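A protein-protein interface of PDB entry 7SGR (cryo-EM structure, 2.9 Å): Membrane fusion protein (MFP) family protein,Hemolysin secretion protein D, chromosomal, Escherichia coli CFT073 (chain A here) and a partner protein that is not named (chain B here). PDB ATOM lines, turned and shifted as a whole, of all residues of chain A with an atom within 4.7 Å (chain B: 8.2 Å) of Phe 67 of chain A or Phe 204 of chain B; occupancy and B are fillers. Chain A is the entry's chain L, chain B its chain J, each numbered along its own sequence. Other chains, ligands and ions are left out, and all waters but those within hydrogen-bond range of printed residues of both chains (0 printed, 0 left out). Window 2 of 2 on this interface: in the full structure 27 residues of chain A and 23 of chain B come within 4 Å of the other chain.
Of the printed residues of chain B, Ile 64 of chain A touches Phe 167, Phe 204 and Ile 207.
Of chain B, only Phe 204 (3.3 Å) comes within 4 Å of Phe 67 of chain A.
Of chain A, only Ile 64 and Phe 67 come within 4 Å of Phe 204 of chain B.
Printed residues of chain A within 4 Å of Ile 207 of chain B: Ile 64 (3.7 Å).
The nearest residue of chain A that does not touch Phe 204 of chain B is Phe 63 of chain A (4.4 Å).
The nearest printed residue of chain A that does not touch Phe 167 of chain B is Met 65 of chain A (5.2 Å).
Of the 9 printed residues of chain A, 5 touch a printed residue of chain B.
Among the printed residues, no Asp or Glu carboxylate lies within 4 Å of a Lys or Arg side-chain nitrogen of the other chain.
Among the printed residues, pairs that only touch across the chains: Phe 67 of chain A with Phe 204 of chain B (3.3 Å), Met 65 of chain A with Phe 163 of chain B (3.5 Å), Leu 68 of chain A with Phe 167 of chain B (3.5 Å), Val 69 of chain A with Phe 163 of chain B (3.7 Å), Ile 64 of chain A with Ile 207 of chain B (3.7 Å), Ile 64 of chain A with Phe 204 of chain B (3.7 Å), Leu 68 of chain A with Phe 163 of chain B (3.9 Å) and Ile 64 of chain A with Phe 167 of chain B (3.96 Å).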
ATOM      1  N   PHE A  63      23.095  -4.046  18.877  1.00  0.00           N
ATOM      2  CA  PHE A  63      22.167  -3.601  17.847  1.00  0.00           C
ATOM      3  C   PHE A  63      21.425  -2.344  18.277  1.00  0.00           C
ATOM      4  O   PHE A  63      21.259  -1.417  17.479  1.00  0.00           O
ATOM      5  CB  PHE A  63      21.183  -4.722  17.512  1.00  0.00           C
ATOM      6  CG  PHE A  63      19.874  -4.239  16.957  1.00  0.00           C
ATOM      7  CD1 PHE A  63      19.795  -3.741  15.667  1.00  0.00           C
ATOM      8  CD2 PHE A  63      18.722  -4.291  17.722  1.00  0.00           C
ATOM      9  CE1 PHE A  63      18.590  -3.299  15.153  1.00  0.00           C
ATOM     10  CE2 PHE A  63      17.514  -3.849  17.214  1.00  0.00           C
ATOM     11  CZ  PHE A  63      17.449  -3.354  15.928  1.00  0.00           C
ATOM     12  N   ILE A  64      20.978  -2.287  19.533  1.00  0.00           N
ATOM     13  CA  ILE A  64      20.290  -1.087  20.010  1.00  0.00           C
ATOM     14  C   ILE A  64      21.231   0.114  19.999  1.00  0.00           C
ATOM     15  O   ILE A  64      20.864   1.213  19.553  1.00  0.00           O
ATOM     16  CB  ILE A  64      19.697  -1.333  21.409  1.00  0.00           C
ATOM     17  CG1 ILE A  64      18.511  -2.292  21.322  1.00  0.00           C
ATOM     18  CG2 ILE A  64      19.281  -0.021  22.051  1.00  0.00           C
ATOM     19  CD1 ILE A  64      17.822  -2.530  22.643  1.00  0.00           C
ATOM     20  N   MET A  65      22.460  -0.075  20.484  1.00  0.00           N
ATOM     21  CA  MET A  65      23.421   1.023  20.532  1.00  0.00           C
ATOM     22  C   MET A  65      23.769   1.509  19.128  1.00  0.00           C
ATOM     23  O   MET A  65      23.835   2.720  18.871  1.00  0.00           O
ATOM     24  CB  MET A  65      24.669   0.562  21.282  1.00  0.00           C
ATOM     25  CG  MET A  65      24.471   0.491  22.787  1.00  0.00           C
ATOM     26  SD  MET A  65      25.513  -0.749  23.571  1.00  0.00           S
ATOM     27  CE  MET A  65      27.007   0.189  23.832  1.00  0.00           C
ATOM     28  N   GLY A  66      23.983   0.574  18.201  1.00  0.00           N
ATOM     29  CA  GLY A  66      24.246   0.947  16.824  1.00  0.00           C
ATOM     30  C   GLY A  66      23.067   1.619  16.156  1.00  0.00           C
ATOM     31  O   GLY A  66      23.252   2.512  15.329  1.00  0.00           O
ATOM     32  N   PHE A  67      21.846   1.201  16.493  1.00  0.00           N
ATOM     33  CA  PHE A  67      20.662   1.872  15.970  1.00  0.00           C
ATOM     34  C   PHE A  67      20.619   3.322  16.429  1.00  0.00           C
ATOM     35  O   PHE A  67      20.336   4.228  15.636  1.00  0.00           O
ATOM     36  CB  PHE A  67      19.401   1.130  16.414  1.00  0.00           C
ATOM     37  CG  PHE A  67      18.192   1.437  15.582  1.00  0.00           C
ATOM     38  CD1 PHE A  67      17.984   0.793  14.374  1.00  0.00           C
ATOM     39  CD2 PHE A  67      17.256   2.362  16.011  1.00  0.00           C
ATOM     40  CE1 PHE A  67      16.869   1.071  13.607  1.00  0.00           C
ATOM     41  CE2 PHE A  67      16.139   2.644  15.249  1.00  0.00           C
ATOM     42  CZ  PHE A  67      15.945   1.998  14.045  1.00  0.00           C
ATOM     43  N   LEU A  68      20.909   3.560  17.711  1.00  0.00           N
ATOM     44  CA  LEU A  68      20.960   4.936  18.200  1.00  0.00           C
ATOM     45  C   LEU A  68      22.037   5.739  17.480  1.00  0.00           C
ATOM     46  O   LEU A  68      21.799   6.883  17.068  1.00  0.00           O
ATOM     47  CB  LEU A  68      21.206   4.959  19.708  1.00  0.00           C
ATOM     48  CG  LEU A  68      21.244   6.364  20.317  1.00  0.00           C
ATOM     49  CD1 LEU A  68      19.870   7.015  20.262  1.00  0.00           C
ATOM     50  CD2 LEU A  68      21.777   6.339  21.742  1.00  0.00           C
ATOM     51  N   VAL A  69      23.225   5.154  17.315  1.00  0.00           N
ATOM     52  CA  VAL A  69      24.324   5.869  16.667  1.00  0.00           C
ATOM     53  C   VAL A  69      23.964   6.204  15.223  1.00  0.00           C
ATOM     54  O   VAL A  69      24.202   7.320  14.745  1.00  0.00           O
ATOM     55  CB  VAL A  69      25.623   5.046  16.750  1.00  0.00           C
ATOM     56  CG1 VAL A  69      26.644   5.554  15.746  1.00  0.00           C
ATOM     57  CG2 VAL A  69      26.188   5.095  18.160  1.00  0.00           C
ATOM     58  N   ILE A  70      23.382   5.238  14.508  1.00  0.00           N
ATOM     59  CA  ILE A  70      22.996   5.450  13.117  1.00  0.00           C
ATOM     60  C   ILE A  70      21.928   6.530  13.018  1.00  0.00           C
ATOM     61  O   ILE A  70      21.985   7.399  12.140  1.00  0.00           O
ATOM     62  CB  ILE A  70      22.528   4.126  12.486  1.00  0.00           C
ATOM     63  CG1 ILE A  70      23.724   3.211  12.216  1.00  0.00           C
ATOM     64  CG2 ILE A  70      21.749   4.382  11.206  1.00  0.00           C
ATOM     65  CD1 ILE A  70      24.682   3.751  11.179  1.00  0.00           C
ATOM     66  N   ALA A  71      20.937   6.495  13.913  1.00  0.00           N
ATOM     67  CA  ALA A  71      19.894   7.514  13.892  1.00  0.00           C
ATOM     68  C   ALA A  71      20.483   8.901  14.112  1.00  0.00           C
ATOM     69  O   ALA A  71      20.144   9.853  13.398  1.00  0.00           O
ATOM     70  CB  ALA A  71      18.833   7.202  14.949  1.00  0.00           C
ATOM     71  N   PHE B 163      25.604   4.794  27.178  1.00  0.00           N
ATOM     72  CA  PHE B 163      24.535   4.845  26.186  1.00  0.00           C
ATOM     73  C   PHE B 163      23.165   4.992  26.838  1.00  0.00           C
ATOM     74  O   PHE B 163      22.291   5.673  26.290  1.00  0.00           O
ATOM     75  CB  PHE B 163      24.580   3.608  25.293  1.00  0.00           C
ATOM     76  CG  PHE B 163      25.356   3.810  24.025  1.00  0.00           C
ATOM     77  CD1 PHE B 163      26.739   3.835  24.039  1.00  0.00           C
ATOM     78  CD2 PHE B 163      24.701   3.993  22.819  1.00  0.00           C
ATOM     79  CE1 PHE B 163      27.455   4.027  22.875  1.00  0.00           C
ATOM     80  CE2 PHE B 163      25.412   4.184  21.652  1.00  0.00           C
ATOM     81  CZ  PHE B 163      26.790   4.202  21.680  1.00  0.00           C
ATOM     82  N   LEU B 164      22.954   4.364  27.997  1.00  0.00           N
ATOM     83  CA  LEU B 164      21.715   4.575  28.740  1.00  0.00           C
ATOM     84  C   LEU B 164      21.583   6.025  29.181  1.00  0.00           C
ATOM     85  O   LEU B 164      20.482   6.588  29.165  1.00  0.00           O
ATOM     86  CB  LEU B 164      21.657   3.648  29.952  1.00  0.00           C
ATOM     87  CG  LEU B 164      21.377   2.172  29.689  1.00  0.00           C
ATOM     88  CD1 LEU B 164      21.561   1.375  30.960  1.00  0.00           C
ATOM     89  CD2 LEU B 164      19.967   2.007  29.161  1.00  0.00           C
ATOM     90  N   PHE B 167      20.450   7.910  26.172  1.00  0.00           N
ATOM     91  CA  PHE B 167      19.037   7.630  25.927  1.00  0.00           C
ATOM     92  C   PHE B 167      18.150   8.416  26.881  1.00  0.00           C
ATOM     93  O   PHE B 167      17.108   8.948  26.480  1.00  0.00           O
ATOM     94  CB  PHE B 167      18.762   6.132  26.073  1.00  0.00           C
ATOM     95  CG  PHE B 167      18.870   5.360  24.790  1.00  0.00           C
ATOM     96  CD1 PHE B 167      17.907   5.492  23.805  1.00  0.00           C
ATOM     97  CD2 PHE B 167      19.920   4.485  24.580  1.00  0.00           C
ATOM     98  CE1 PHE B 167      17.999   4.775  22.629  1.00  0.00           C
ATOM     99  CE2 PHE B 167      20.017   3.765  23.406  1.00  0.00           C
ATOM    100  CZ  PHE B 167      19.055   3.911  22.429  1.00  0.00           C
ATOM    101  N   ALA B 197       9.167   8.894  17.513  1.00  0.00           N
ATOM    102  CA  ALA B 197      10.562   8.706  17.899  1.00  0.00           C
ATOM    103  C   ALA B 197      10.688   8.352  19.376  1.00  0.00           C
ATOM    104  O   ALA B 197      11.475   7.468  19.743  1.00  0.00           O
ATOM    105  CB  ALA B 197      11.370   9.963  17.579  1.00  0.00           C
ATOM    106  N   LEU B 198       9.910   9.023  20.230  1.00  0.00           N
ATOM    107  CA  LEU B 198       9.995   8.794  21.666  1.00  0.00           C
ATOM    108  C   LEU B 198       9.585   7.379  22.036  1.00  0.00           C
ATOM    109  O   LEU B 198      10.172   6.790  22.947  1.00  0.00           O
ATOM    110  CB  LEU B 198       9.126   9.808  22.408  1.00  0.00           C
ATOM    111  CG  LEU B 198       9.470  10.059  23.876  1.00  0.00           C
ATOM    112  CD1 LEU B 198      10.841  10.691  24.006  1.00  0.00           C
ATOM    113  CD2 LEU B 198       8.411  10.931  24.529  1.00  0.00           C
ATOM    114  N   SER B 199       8.584   6.820  21.355  1.00  0.00           N
ATOM    115  CA  SER B 199       8.154   5.461  21.681  1.00  0.00           C
ATOM    116  C   SER B 199       9.297   4.463  21.509  1.00  0.00           C
ATOM    117  O   SER B 199       9.602   3.681  22.422  1.00  0.00           O
ATOM    118  CB  SER B 199       6.958   5.068  20.813  1.00  0.00           C
ATOM    119  OG  SER B 199       5.838   5.888  21.092  1.00  0.00           O
ATOM    120  N   VAL B 200       9.953   4.486  20.347  1.00  0.00           N
ATOM    121  CA  VAL B 200      11.040   3.545  20.103  1.00  0.00           C
ATOM    122  C   VAL B 200      12.241   3.860  20.988  1.00  0.00           C
ATOM    123  O   VAL B 200      12.934   2.941  21.445  1.00  0.00           O
ATOM    124  CB  VAL B 200      11.412   3.513  18.607  1.00  0.00           C
ATOM    125  CG1 VAL B 200      10.167   3.298  17.760  1.00  0.00           C
ATOM    126  CG2 VAL B 200      12.132   4.783  18.182  1.00  0.00           C
ATOM    127  N   VAL B 201      12.506   5.143  21.263  1.00  0.00           N
ATOM    128  CA  VAL B 201      13.609   5.485  22.157  1.00  0.00           C
ATOM    129  C   VAL B 201      13.373   4.890  23.539  1.00  0.00           C
ATOM    130  O   VAL B 201      14.279   4.305  24.144  1.00  0.00           O
ATOM    131  CB  VAL B 201      13.797   7.011  22.220  1.00  0.00           C
ATOM    132  CG1 VAL B 201      14.652   7.391  23.416  1.00  0.00           C
ATOM    133  CG2 VAL B 201      14.437   7.514  20.939  1.00  0.00           C
ATOM    134  N   VAL B 202      12.148   5.016  24.051  1.00  0.00           N
ATOM    135  CA  VAL B 202      11.818   4.472  25.364  1.00  0.00           C
ATOM    136  C   VAL B 202      11.946   2.955  25.374  1.00  0.00           C
ATOM    137  O   VAL B 202      12.502   2.369  26.312  1.00  0.00           O
ATOM    138  CB  VAL B 202      10.408   4.914  25.787  1.00  0.00           C
ATOM    139  CG1 VAL B 202      10.031   4.206  27.045  1.00  0.00           C
ATOM    140  CG2 VAL B 202      10.378   6.413  26.020  1.00  0.00           C
ATOM    141  N   VAL B 203      11.406   2.290  24.349  1.00  0.00           N
ATOM    142  CA  VAL B 203      11.471   0.829  24.323  1.00  0.00           C
ATOM    143  C   VAL B 203      12.922   0.364  24.308  1.00  0.00           C
ATOM    144  O   VAL B 203      13.310  -0.552  25.051  1.00  0.00           O
ATOM    145  CB  VAL B 203      10.682   0.277  23.122  1.00  0.00           C
ATOM    146  CG1 VAL B 203      10.930  -1.213  22.964  1.00  0.00           C
ATOM    147  CG2 VAL B 203       9.199   0.549  23.297  1.00  0.00           C
ATOM    148  N   PHE B 204      13.750   1.003  23.480  1.00  0.00           N
ATOM    149  CA  PHE B 204      15.155   0.625  23.402  1.00  0.00           C
ATOM    150  C   PHE B 204      15.872   0.894  24.718  1.00  0.00           C
ATOM    151  O   PHE B 204      16.717   0.100  25.143  1.00  0.00           O
ATOM    152  CB  PHE B 204      15.830   1.367  22.251  1.00  0.00           C
ATOM    153  CG  PHE B 204      15.561   0.761  20.902  1.00  0.00           C
ATOM    154  CD1 PHE B 204      14.536  -0.155  20.731  1.00  0.00           C
ATOM    155  CD2 PHE B 204      16.330   1.106  19.806  1.00  0.00           C
ATOM    156  CE1 PHE B 204      14.285  -0.714  19.495  1.00  0.00           C
ATOM    157  CE2 PHE B 204      16.084   0.549  18.569  1.00  0.00           C
ATOM    158  CZ  PHE B 204      15.060  -0.361  18.413  1.00  0.00           C
ATOM    159  N   GLU B 205      15.547   2.007  25.380  1.00  0.00           N
ATOM    160  CA  GLU B 205      16.170   2.310  26.665  1.00  0.00           C
ATOM    161  C   GLU B 205      15.809   1.268  27.716  1.00  0.00           C
ATOM    162  O   GLU B 205      16.670   0.841  28.494  1.00  0.00           O
ATOM    163  CB  GLU B 205      15.757   3.706  27.129  1.00  0.00           C
ATOM    164  CG  GLU B 205      16.330   4.109  28.474  1.00  0.00           C
ATOM    165  CD  GLU B 205      15.531   5.212  29.139  1.00  0.00           C
ATOM    166  OE1 GLU B 205      14.354   5.403  28.765  1.00  0.00           O
ATOM    167  OE2 GLU B 205      16.078   5.887  30.036  1.00  0.00           O
ATOM    168  N   ILE B 206      14.543   0.846  27.754  1.00  0.00           N
ATOM    169  CA  ILE B 206      14.125  -0.170  28.720  1.00  0.00           C
ATOM    170  C   ILE B 206      14.856  -1.483  28.463  1.00  0.00           C
ATOM    171  O   ILE B 206      15.379  -2.119  29.390  1.00  0.00           O
ATOM    172  CB  ILE B 206      12.597  -0.357  28.679  1.00  0.00           C
ATOM    173  CG1 ILE B 206      11.888   0.949  29.038  1.00  0.00           C
ATOM    174  CG2 ILE B 206      12.167  -1.479  29.605  1.00  0.00           C
ATOM    175  CD1 ILE B 206      12.222   1.463  30.418  1.00  0.00           C
ATOM    176  N   ILE B 207      14.912  -1.901  27.195  1.00  0.00           N
ATOM    177  CA  ILE B 207      15.592  -3.153  26.868  1.00  0.00           C
ATOM    178  C   ILE B 207      17.071  -3.069  27.226  1.00  0.00           C
ATOM    179  O   ILE B 207      17.645  -4.015  27.779  1.00  0.00           O
ATOM    180  CB  ILE B 207      15.387  -3.508  25.383  1.00  0.00           C
ATOM    181  CG1 ILE B 207      13.898  -3.634  25.064  1.00  0.00           C
ATOM    182  CG2 ILE B 207      16.108  -4.798  25.041  1.00  0.00           C
ATOM    183  CD1 ILE B 207      13.198  -4.715  25.847  1.00  0.00           C
ATOM    184  N   LEU B 208      17.707  -1.937  26.922  1.00  0.00           N
ATOM    185  CA  LEU B 208      19.132  -1.785  27.195  1.00  0.00           C
ATOM    186  C   LEU B 208      19.416  -1.785  28.692  1.00  0.00           C
ATOM    187  O   LEU B 208      20.410  -2.369  29.138  1.00  0.00           O
ATOM    188  CB  LEU B 208      19.647  -0.503  26.545  1.00  0.00           C
ATOM    189  CG  LEU B 208      21.162  -0.323  26.462  1.00  0.00           C
ATOM    190  CD1 LEU B 208      21.781  -1.443  25.650  1.00  0.00           C
ATOM    191  CD2 LEU B 208      21.503   1.027  25.859  1.00  0.00           C
ATOM    192  N   SER B 209      18.560  -1.135  29.485  1.00  0.00           N
ATOM    193  CA  SER B 209      18.746  -1.149  30.933  1.00  0.00           C
ATOM    194  C   SER B 209      18.594  -2.556  31.495  1.00  0.00           C
ATOM    195  O   SER B 209      19.389  -2.980  32.348  1.00  0.00           O
ATOM    196  CB  SER B 209      17.756  -0.195  31.597  1.00  0.00           C
ATOM    197  OG  SER B 209      17.974  -0.134  32.994  1.00  0.00           O
ATOM    198  N   GLY B 210      17.587  -3.297  31.028  1.00  0.00           N
ATOM    199  CA  GLY B 210      17.443  -4.676  31.465  1.00  0.00           C
ATOM    200  C   GLY B 210      18.646  -5.526  31.106  1.00  0.00           C
ATOM    201  O   GLY B 210      19.126  -6.322  31.921  1.00  0.00           O
ATOM    202  N   LEU B 211      19.160  -5.358  29.885  1.00  0.00           N
ATOM    203  CA  LEU B 211      20.330  -6.120  29.462  1.00  0.00           C
ATOM    204  C   LEU B 211      21.555  -5.773  30.298  1.00  0.00           C
ATOM    205  O   LEU B 211      22.332  -6.661  30.663  1.00  0.00           O
ATOM    206  CB  LEU B 211      20.610  -5.874  27.981  1.00  0.00           C
ATOM    207  CG  LEU B 211      19.646  -6.529  26.993  1.00  0.00           C
ATOM    208  CD1 LEU B 211      20.086  -6.245  25.571  1.00  0.00           C
ATOM    209  CD2 LEU B 211      19.551  -8.023  27.241  1.00  0.00           C
